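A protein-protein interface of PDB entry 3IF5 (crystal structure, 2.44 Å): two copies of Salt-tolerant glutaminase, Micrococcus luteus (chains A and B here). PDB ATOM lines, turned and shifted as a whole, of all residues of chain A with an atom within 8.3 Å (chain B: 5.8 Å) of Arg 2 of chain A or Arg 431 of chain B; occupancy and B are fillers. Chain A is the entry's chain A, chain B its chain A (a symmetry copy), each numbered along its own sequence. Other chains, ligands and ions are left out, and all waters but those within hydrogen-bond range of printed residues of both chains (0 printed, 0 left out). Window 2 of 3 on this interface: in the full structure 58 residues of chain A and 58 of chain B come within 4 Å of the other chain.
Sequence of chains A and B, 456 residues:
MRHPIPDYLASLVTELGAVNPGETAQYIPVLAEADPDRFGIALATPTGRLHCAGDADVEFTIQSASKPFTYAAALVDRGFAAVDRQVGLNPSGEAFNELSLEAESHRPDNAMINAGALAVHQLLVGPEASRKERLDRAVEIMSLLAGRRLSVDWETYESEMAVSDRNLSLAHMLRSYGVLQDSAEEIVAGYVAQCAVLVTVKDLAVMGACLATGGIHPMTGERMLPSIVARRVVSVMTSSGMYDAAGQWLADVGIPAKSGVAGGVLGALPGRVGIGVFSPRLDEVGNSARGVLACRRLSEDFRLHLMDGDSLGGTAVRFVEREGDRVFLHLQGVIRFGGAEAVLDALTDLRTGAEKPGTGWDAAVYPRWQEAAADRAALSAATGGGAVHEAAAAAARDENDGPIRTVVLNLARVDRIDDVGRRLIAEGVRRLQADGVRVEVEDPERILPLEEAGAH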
ATOM      1  N   MET A   1     -10.433 -25.143 -20.053  1.00  0.00           N
ATOM      2  CA  MET A   1      -9.532 -24.924 -21.218  1.00  0.00           C
ATOM      3  C   MET A   1      -8.742 -23.636 -21.022  1.00  0.00           C
ATOM      4  O   MET A   1      -9.016 -22.870 -20.098  1.00  0.00           O
ATOM      5  CB  MET A   1     -10.349 -24.831 -22.510  1.00  0.00           C
ATOM      6  CG  MET A   1     -11.419 -23.741 -22.507  1.00  0.00           C
ATOM      7  SD  MET A   1     -12.133 -23.540 -24.143  1.00  0.00           S
ATOM      8  CE  MET A   1     -11.056 -22.304 -24.827  1.00  0.00           C
ATOM      9  N   ARG A   2      -7.753 -23.407 -21.882  1.00  0.00           N
ATOM     10  CA  ARG A   2      -6.954 -22.187 -21.799  1.00  0.00           C
ATOM     11  C   ARG A   2      -7.420 -21.261 -22.915  1.00  0.00           C
ATOM     12  O   ARG A   2      -7.897 -21.716 -23.957  1.00  0.00           O
ATOM     13  CB  ARG A   2      -5.465 -22.497 -21.954  1.00  0.00           C
ATOM     14  CG  ARG A   2      -5.064 -22.953 -23.342  1.00  0.00           C
ATOM     15  CD  ARG A   2      -3.589 -23.308 -23.392  1.00  0.00           C
ATOM     16  NE  ARG A   2      -2.766 -22.245 -22.824  1.00  0.00           N
ATOM     17  CZ  ARG A   2      -1.444 -22.185 -22.920  1.00  0.00           C
ATOM     18  NH1 ARG A   2      -0.773 -23.130 -23.571  1.00  0.00           N
ATOM     19  NH2 ARG A   2      -0.790 -21.175 -22.362  1.00  0.00           N
ATOM     20  N   HIS A   3      -7.294 -19.959 -22.698  1.00  0.00           N
ATOM     21  CA  HIS A   3      -7.727 -18.999 -23.695  1.00  0.00           C
ATOM     22  C   HIS A   3      -6.791 -19.029 -24.908  1.00  0.00           C
ATOM     23  O   HIS A   3      -5.572 -18.934 -24.773  1.00  0.00           O
ATOM     24  CB  HIS A   3      -7.791 -17.605 -23.071  1.00  0.00           C
ATOM     25  CG  HIS A   3      -8.746 -16.688 -23.761  1.00  0.00           C
ATOM     26  ND1 HIS A   3      -8.520 -16.197 -25.027  1.00  0.00           N
ATOM     27  CD2 HIS A   3      -9.957 -16.212 -23.383  1.00  0.00           C
ATOM     28  CE1 HIS A   3      -9.551 -15.462 -25.402  1.00  0.00           C
ATOM     29  NE2 HIS A   3     -10.437 -15.455 -24.422  1.00  0.00           N
ATOM     30  N   PRO A   4      -7.356 -19.171 -26.116  1.00  0.00           N
ATOM     31  CA  PRO A   4      -6.531 -19.214 -27.328  1.00  0.00           C
ATOM     32  C   PRO A   4      -5.806 -17.951 -27.798  1.00  0.00           C
ATOM     33  O   PRO A   4      -4.783 -18.058 -28.476  1.00  0.00           O
ATOM     34  CB  PRO A   4      -7.493 -19.766 -28.384  1.00  0.00           C
ATOM     35  CG  PRO A   4      -8.827 -19.315 -27.901  1.00  0.00           C
ATOM     36  CD  PRO A   4      -8.747 -19.544 -26.415  1.00  0.00           C
ATOM     37  N   ILE A   5      -6.309 -16.764 -27.448  1.00  0.00           N
ATOM     38  CA  ILE A   5      -5.659 -15.524 -27.897  1.00  0.00           C
ATOM     39  C   ILE A   5      -4.217 -15.371 -27.417  1.00  0.00           C
ATOM     40  O   ILE A   5      -3.324 -15.114 -28.219  1.00  0.00           O
ATOM     41  CB  ILE A   5      -6.471 -14.250 -27.494  1.00  0.00           C
ATOM     42  CG1 ILE A   5      -7.597 -13.996 -28.500  1.00  0.00           C
ATOM     43  CG2 ILE A   5      -5.562 -13.022 -27.501  1.00  0.00           C
ATOM     44  CD1 ILE A   5      -8.583 -15.125 -28.636  1.00  0.00           C
ATOM     45  N   PRO A   6      -3.967 -15.514 -26.109  1.00  0.00           N
ATOM     46  CA  PRO A   6      -2.571 -15.363 -25.681  1.00  0.00           C
ATOM     47  C   PRO A   6      -1.631 -16.338 -26.390  1.00  0.00           C
ATOM     48  O   PRO A   6      -0.437 -16.072 -26.528  1.00  0.00           O
ATOM     49  CB  PRO A   6      -2.632 -15.555 -24.154  1.00  0.00           C
ATOM     50  CG  PRO A   6      -3.956 -16.215 -23.897  1.00  0.00           C
ATOM     51  CD  PRO A   6      -4.875 -15.666 -24.957  1.00  0.00           C
ATOM     52  N   ASP A   7      -2.169 -17.461 -26.860  1.00  0.00           N
ATOM     53  CA  ASP A   7      -1.350 -18.423 -27.587  1.00  0.00           C
ATOM     54  C   ASP A   7      -1.134 -17.926 -29.009  1.00  0.00           C
ATOM     55  O   ASP A   7      -0.059 -18.113 -29.587  1.00  0.00           O
ATOM     56  CB  ASP A   7      -2.005 -19.806 -27.605  1.00  0.00           C
ATOM     57  CG  ASP A   7      -1.890 -20.508 -26.277  1.00  0.00           C
ATOM     58  OD1 ASP A   7      -0.786 -20.480 -25.701  1.00  0.00           O
ATOM     59  OD2 ASP A   7      -2.890 -21.089 -25.809  1.00  0.00           O
ATOM     60  N   TYR A   8      -2.154 -17.299 -29.585  1.00  0.00           N
ATOM     61  CA  TYR A   8      -2.000 -16.762 -30.923  1.00  0.00           C
ATOM     62  C   TYR A   8      -0.891 -15.706 -30.847  1.00  0.00           C
ATOM     63  O   TYR A   8       0.004 -15.662 -31.696  1.00  0.00           O
ATOM     64  CB  TYR A   8      -3.297 -16.117 -31.408  1.00  0.00           C
ATOM     65  CG  TYR A   8      -3.082 -15.135 -32.540  1.00  0.00           C
ATOM     66  CD1 TYR A   8      -2.994 -15.565 -33.863  1.00  0.00           C
ATOM     67  CD2 TYR A   8      -2.899 -13.775 -32.273  1.00  0.00           C
ATOM     68  CE1 TYR A   8      -2.729 -14.663 -34.900  1.00  0.00           C
ATOM     69  CE2 TYR A   8      -2.632 -12.871 -33.293  1.00  0.00           C
ATOM     70  CZ  TYR A   8      -2.546 -13.318 -34.602  1.00  0.00           C
ATOM     71  OH  TYR A   8      -2.276 -12.409 -35.603  1.00  0.00           O
ATOM     72  N   ALA A  10       1.549 -15.536 -28.761  1.00  0.00           N
ATOM     73  CA  ALA A  10       2.819 -16.220 -28.558  1.00  0.00           C
ATOM     74  C   ALA A  10       3.383 -16.684 -29.899  1.00  0.00           C
ATOM     75  O   ALA A  10       4.591 -16.647 -30.116  1.00  0.00           O
ATOM     76  CB  ALA A  10       2.637 -17.415 -27.627  1.00  0.00           C
ATOM     77  N   SER A  11       2.506 -17.119 -30.797  1.00  0.00           N
ATOM     78  CA  SER A  11       2.938 -17.566 -32.115  1.00  0.00           C
ATOM     79  C   SER A  11       3.516 -16.401 -32.898  1.00  0.00           C
ATOM     80  O   SER A  11       4.574 -16.528 -33.520  1.00  0.00           O
ATOM     81  CB  SER A  11       1.768 -18.167 -32.896  1.00  0.00           C
ATOM     82  OG  SER A  11       1.294 -19.342 -32.271  1.00  0.00           O
ATOM     83  N   CYS A  52      -1.411 -11.371 -23.357  1.00  0.00           N
ATOM     84  CA  CYS A  52      -0.082 -10.948 -23.774  1.00  0.00           C
ATOM     85  C   CYS A  52       0.855 -12.116 -24.063  1.00  0.00           C
ATOM     86  O   CYS A  52       0.492 -13.279 -23.885  1.00  0.00           O
ATOM     87  CB  CYS A  52       0.529 -10.036 -22.714  1.00  0.00           C
ATOM     88  SG  CYS A  52       0.537 -10.735 -21.069  1.00  0.00           S
ATOM     89  N   THR B 348     -13.339 -20.562 -21.117  1.00  0.00           N
ATOM     90  CA  THR B 348     -12.198 -20.626 -20.214  1.00  0.00           C
ATOM     91  C   THR B 348     -12.656 -20.442 -18.767  1.00  0.00           C
ATOM     92  O   THR B 348     -12.095 -21.044 -17.852  1.00  0.00           O
ATOM     93  CB  THR B 348     -11.154 -19.540 -20.570  1.00  0.00           C
ATOM     94  OG1 THR B 348     -10.782 -19.675 -21.945  1.00  0.00           O
ATOM     95  CG2 THR B 348      -9.905 -19.686 -19.713  1.00  0.00           C
ATOM     96  N   ALA B 426     -14.411 -22.411 -33.229  1.00  0.00           N
ATOM     97  CA  ALA B 426     -14.069 -23.787 -33.591  1.00  0.00           C
ATOM     98  C   ALA B 426     -12.874 -24.245 -32.763  1.00  0.00           C
ATOM     99  O   ALA B 426     -12.790 -25.408 -32.380  1.00  0.00           O
ATOM    100  CB  ALA B 426     -13.733 -23.875 -35.080  1.00  0.00           C
ATOM    101  N   GLU B 427     -11.954 -23.323 -32.491  1.00  0.00           N
ATOM    102  CA  GLU B 427     -10.761 -23.630 -31.705  1.00  0.00           C
ATOM    103  C   GLU B 427     -11.132 -23.862 -30.249  1.00  0.00           C
ATOM    104  O   GLU B 427     -10.566 -24.725 -29.581  1.00  0.00           O
ATOM    105  CB  GLU B 427      -9.755 -22.479 -31.818  1.00  0.00           C
ATOM    106  CG  GLU B 427      -8.543 -22.557 -30.889  1.00  0.00           C
ATOM    107  CD  GLU B 427      -7.677 -23.787 -31.110  1.00  0.00           C
ATOM    108  OE1 GLU B 427      -7.530 -24.222 -32.273  1.00  0.00           O
ATOM    109  OE2 GLU B 427      -7.123 -24.305 -30.116  1.00  0.00           O
ATOM    110  N   GLY B 428     -12.091 -23.086 -29.757  1.00  0.00           N
ATOM    111  CA  GLY B 428     -12.525 -23.235 -28.380  1.00  0.00           C
ATOM    112  C   GLY B 428     -13.207 -24.571 -28.161  1.00  0.00           C
ATOM    113  O   GLY B 428     -13.217 -25.100 -27.052  1.00  0.00           O
ATOM    114  N   VAL B 429     -13.790 -25.117 -29.224  1.00  0.00           N
ATOM    115  CA  VAL B 429     -14.473 -26.400 -29.142  1.00  0.00           C
ATOM    116  C   VAL B 429     -13.434 -27.512 -29.090  1.00  0.00           C
ATOM    117  O   VAL B 429     -13.539 -28.436 -28.284  1.00  0.00           O
ATOM    118  CB  VAL B 429     -15.395 -26.618 -30.356  1.00  0.00           C
ATOM    119  CG1 VAL B 429     -16.035 -27.995 -30.285  1.00  0.00           C
ATOM    120  CG2 VAL B 429     -16.470 -25.538 -30.387  1.00  0.00           C
ATOM    121  N   ARG B 430     -12.426 -27.411 -29.951  1.00  0.00           N
ATOM    122  CA  ARG B 430     -11.341 -28.387 -30.001  1.00  0.00           C
ATOM    123  C   ARG B 430     -10.710 -28.488 -28.612  1.00  0.00           C
ATOM    124  O   ARG B 430     -10.514 -29.584 -28.083  1.00  0.00           O
ATOM    125  CB  ARG B 430     -10.286 -27.941 -31.014  1.00  0.00           C
ATOM    126  CG  ARG B 430      -9.019 -28.788 -31.043  1.00  0.00           C
ATOM    127  CD  ARG B 430      -7.788 -27.923 -31.345  1.00  0.00           C
ATOM    128  NE  ARG B 430      -6.527 -28.620 -31.082  1.00  0.00           N
ATOM    129  CZ  ARG B 430      -5.355 -28.010 -30.913  1.00  0.00           C
ATOM    130  NH1 ARG B 430      -5.281 -26.688 -30.971  1.00  0.00           N
ATOM    131  NH2 ARG B 430      -4.256 -28.720 -30.682  1.00  0.00           N
ATOM    132  N   ARG B 431     -10.409 -27.338 -28.017  1.00  0.00           N
ATOM    133  CA  ARG B 431      -9.793 -27.302 -26.699  1.00  0.00           C
ATOM    134  C   ARG B 431     -10.676 -27.864 -25.606  1.00  0.00           C
ATOM    135  O   ARG B 431     -10.189 -28.527 -24.700  1.00  0.00           O
ATOM    136  CB  ARG B 431      -9.367 -25.870 -26.344  1.00  0.00           C
ATOM    137  CG  ARG B 431      -8.398 -25.274 -27.334  1.00  0.00           C
ATOM    138  CD  ARG B 431      -7.737 -24.019 -26.802  1.00  0.00           C
ATOM    139  NE  ARG B 431      -6.708 -23.545 -27.720  1.00  0.00           N
ATOM    140  CZ  ARG B 431      -5.754 -22.682 -27.393  1.00  0.00           C
ATOM    141  NH1 ARG B 431      -5.696 -22.193 -26.159  1.00  0.00           N
ATOM    142  NH2 ARG B 431      -4.860 -22.305 -28.295  1.00  0.00           N
ATOM    143  N   LEU B 432     -11.969 -27.581 -25.672  1.00  0.00           N
ATOM    144  CA  LEU B 432     -12.888 -28.089 -24.659  1.00  0.00           C
ATOM    145  C   LEU B 432     -12.887 -29.614 -24.696  1.00  0.00           C
ATOM    146  O   LEU B 432     -12.777 -30.284 -23.660  1.00  0.00           O
ATOM    147  CB  LEU B 432     -14.304 -27.586 -24.907  1.00  0.00           C
ATOM    148  CG  LEU B 432     -14.746 -26.369 -24.104  1.00  0.00           C
ATOM    149  CD1 LEU B 432     -16.189 -26.028 -24.466  1.00  0.00           C
ATOM    150  CD2 LEU B 432     -14.621 -26.670 -22.614  1.00  0.00           C
ATOM    151  N   GLN B 433     -13.002 -30.159 -25.902  1.00  0.00           N
ATOM    152  CA  GLN B 433     -13.013 -31.602 -26.089  1.00  0.00           C
ATOM    153  C   GLN B 433     -11.724 -32.233 -25.573  1.00  0.00           C
ATOM    154  O   GLN B 433     -11.750 -33.311 -24.975  1.00  0.00           O
ATOM    155  CB  GLN B 433     -13.202 -31.925 -27.571  1.00  0.00           C
ATOM    156  CG  GLN B 433     -14.481 -31.363 -28.152  1.00  0.00           C
ATOM    157  CD  GLN B 433     -14.649 -31.689 -29.616  1.00  0.00           C
ATOM    158  OE1 GLN B 433     -13.756 -31.442 -30.427  1.00  0.00           O
ATOM    159  NE2 GLN B 433     -15.804 -32.237 -29.971  1.00  0.00           N
ATOM    160  N   ALA B 434     -10.604 -31.557 -25.810  1.00  0.00           N
ATOM    161  CA  ALA B 434      -9.311 -32.048 -25.364  1.00  0.00           C
ATOM    162  C   ALA B 434      -9.239 -32.145 -23.843  1.00  0.00           C
ATOM    163  O   ALA B 434      -8.402 -32.859 -23.305  1.00  0.00           O
ATOM    164  CB  ALA B 434      -8.206 -31.150 -25.890  1.00  0.00           C
ATOM    165  N   ASP B 435     -10.109 -31.414 -23.151  1.00  0.00           N
ATOM    166  CA  ASP B 435     -10.155 -31.451 -21.688  1.00  0.00           C
ATOM    167  C   ASP B 435     -11.051 -32.604 -21.265  1.00  0.00           C
ATOM    168  O   ASP B 435     -11.479 -32.678 -20.111  1.00  0.00           O
ATOM    169  CB  ASP B 435     -10.738 -30.161 -21.105  1.00  0.00           C
ATOM    170  CG  ASP B 435      -9.751 -29.016 -21.094  1.00  0.00           C
ATOM    171  OD1 ASP B 435      -8.666 -29.154 -20.487  1.00  0.00           O
ATOM    172  OD2 ASP B 435     -10.070 -27.966 -21.690  1.00  0.00           O
ATOM    173  N   GLY B 436     -11.342 -33.491 -22.208  1.00  0.00           N
ATOM    174  CA  GLY B 436     -12.195 -34.626 -21.922  1.00  0.00           C
ATOM    175  C   GLY B 436     -13.647 -34.216 -21.755  1.00  0.00           C
ATOM    176  O   GLY B 436     -14.428 -34.920 -21.111  1.00  0.00           O
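Among the printed residues, pairs that only touch across the chains: Met 1 of chain A with Thr 348 of chain B (3.3 Å), Met 1 of chain A with Leu 432 of chain B (3.9 Å), Arg 2 of chain A with Thr 348 of chain B (3.8 Å), His 3 of chain A with Thr 348 of chain B (3.6 Å), His 3 of chain A with Arg 431 of chain B (3.5 Å) and Pro 4 of chain A with Glu 427 of chain B (3.9 Å).
No position is printed for both chains.
Of the 11 pairs that touch across the chains among the printed residues, none has its exchanged pair printed and touching as well.
Of chain B, only Thr 348 and Arg 431 come within 4 Å of Arg 2 of chain A.
Of chain A, only Arg 2 (3.0 Å), His 3 (3.5 Å), Pro 4 (3.3 Å) and Asp 7 (3.0 Å) come within 4 Å of Arg 431 of chain B.
Of the printed residues of chain B, His 3 of chain A touches Thr 348 and Arg 431.
Of the printed residues of chain A, Glu 427 of chain B touches Pro 4 (3.9 Å).
Pro 6 of chain A touches none of the printed residues of chain B.
The nearest residue of chain A that does not touch Arg 431 of chain B is Met 1 of chain A (4.1 Å).
OE2 of Glu 427 of chain B is in salt-bridge range of NE of Arg 431 of chain B (2.5 Å).
The backbone carbonyl oxygen (O) of Asp 7 of chain A is in hydrogen-bond range of the side-chain hydroxyl (OG) of Ser 11 of chain A (3.2 Å).
The backbone NH (N) of Ile 5 of chain A sits at hydrogen-bond distance from a ring nitrogen (ND1) of His 3 of chain A.
The side-chain carboxylate of Asp 7 of chain A lies within salt-bridge range of the guanidinium group of Arg 2 of chain A (3.2 Å).
NH1 of Arg 430 of chain B is in salt-bridge range of OE2 of Glu 427 of chain B, 3.1 Å away.
Hydrophobic or aromatic side chains of chain A within 4 Å of the printed part of chain B: Met 1, His 3 and Pro 4.
Of the 12 printed residues of chain B, 6 touch a printed residue of chain A.
Hydrophobic or aromatic side chains of chain B that line the printed part of chain A: Leu 432.
The backbone NH (N) of Met 1 of chain A lies close to the side-chain carboxylate (OD2) of Asp 435 of chain B, at 3.3 Å.
The side-chain sulfur (SD) of Met 1 of chain A lies close to the backbone carbonyl oxygen (O) of Gly 428 of chain B, at 3.5 Å.
The side-chain carboxylate of Asp 7 of chain A lies within salt-bridge range of the guanidinium group of Arg 431 of chain B (3.0 Å).
The backbone carbonyl oxygen (O) of Arg 2 of chain A lies close to the guanidinium group (NH1) of Arg 431 of chain B (3.1 Å).
N of Pro 4 of chain A sits close to NH1 of Arg 431 of chain B, at 3.4 Å.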
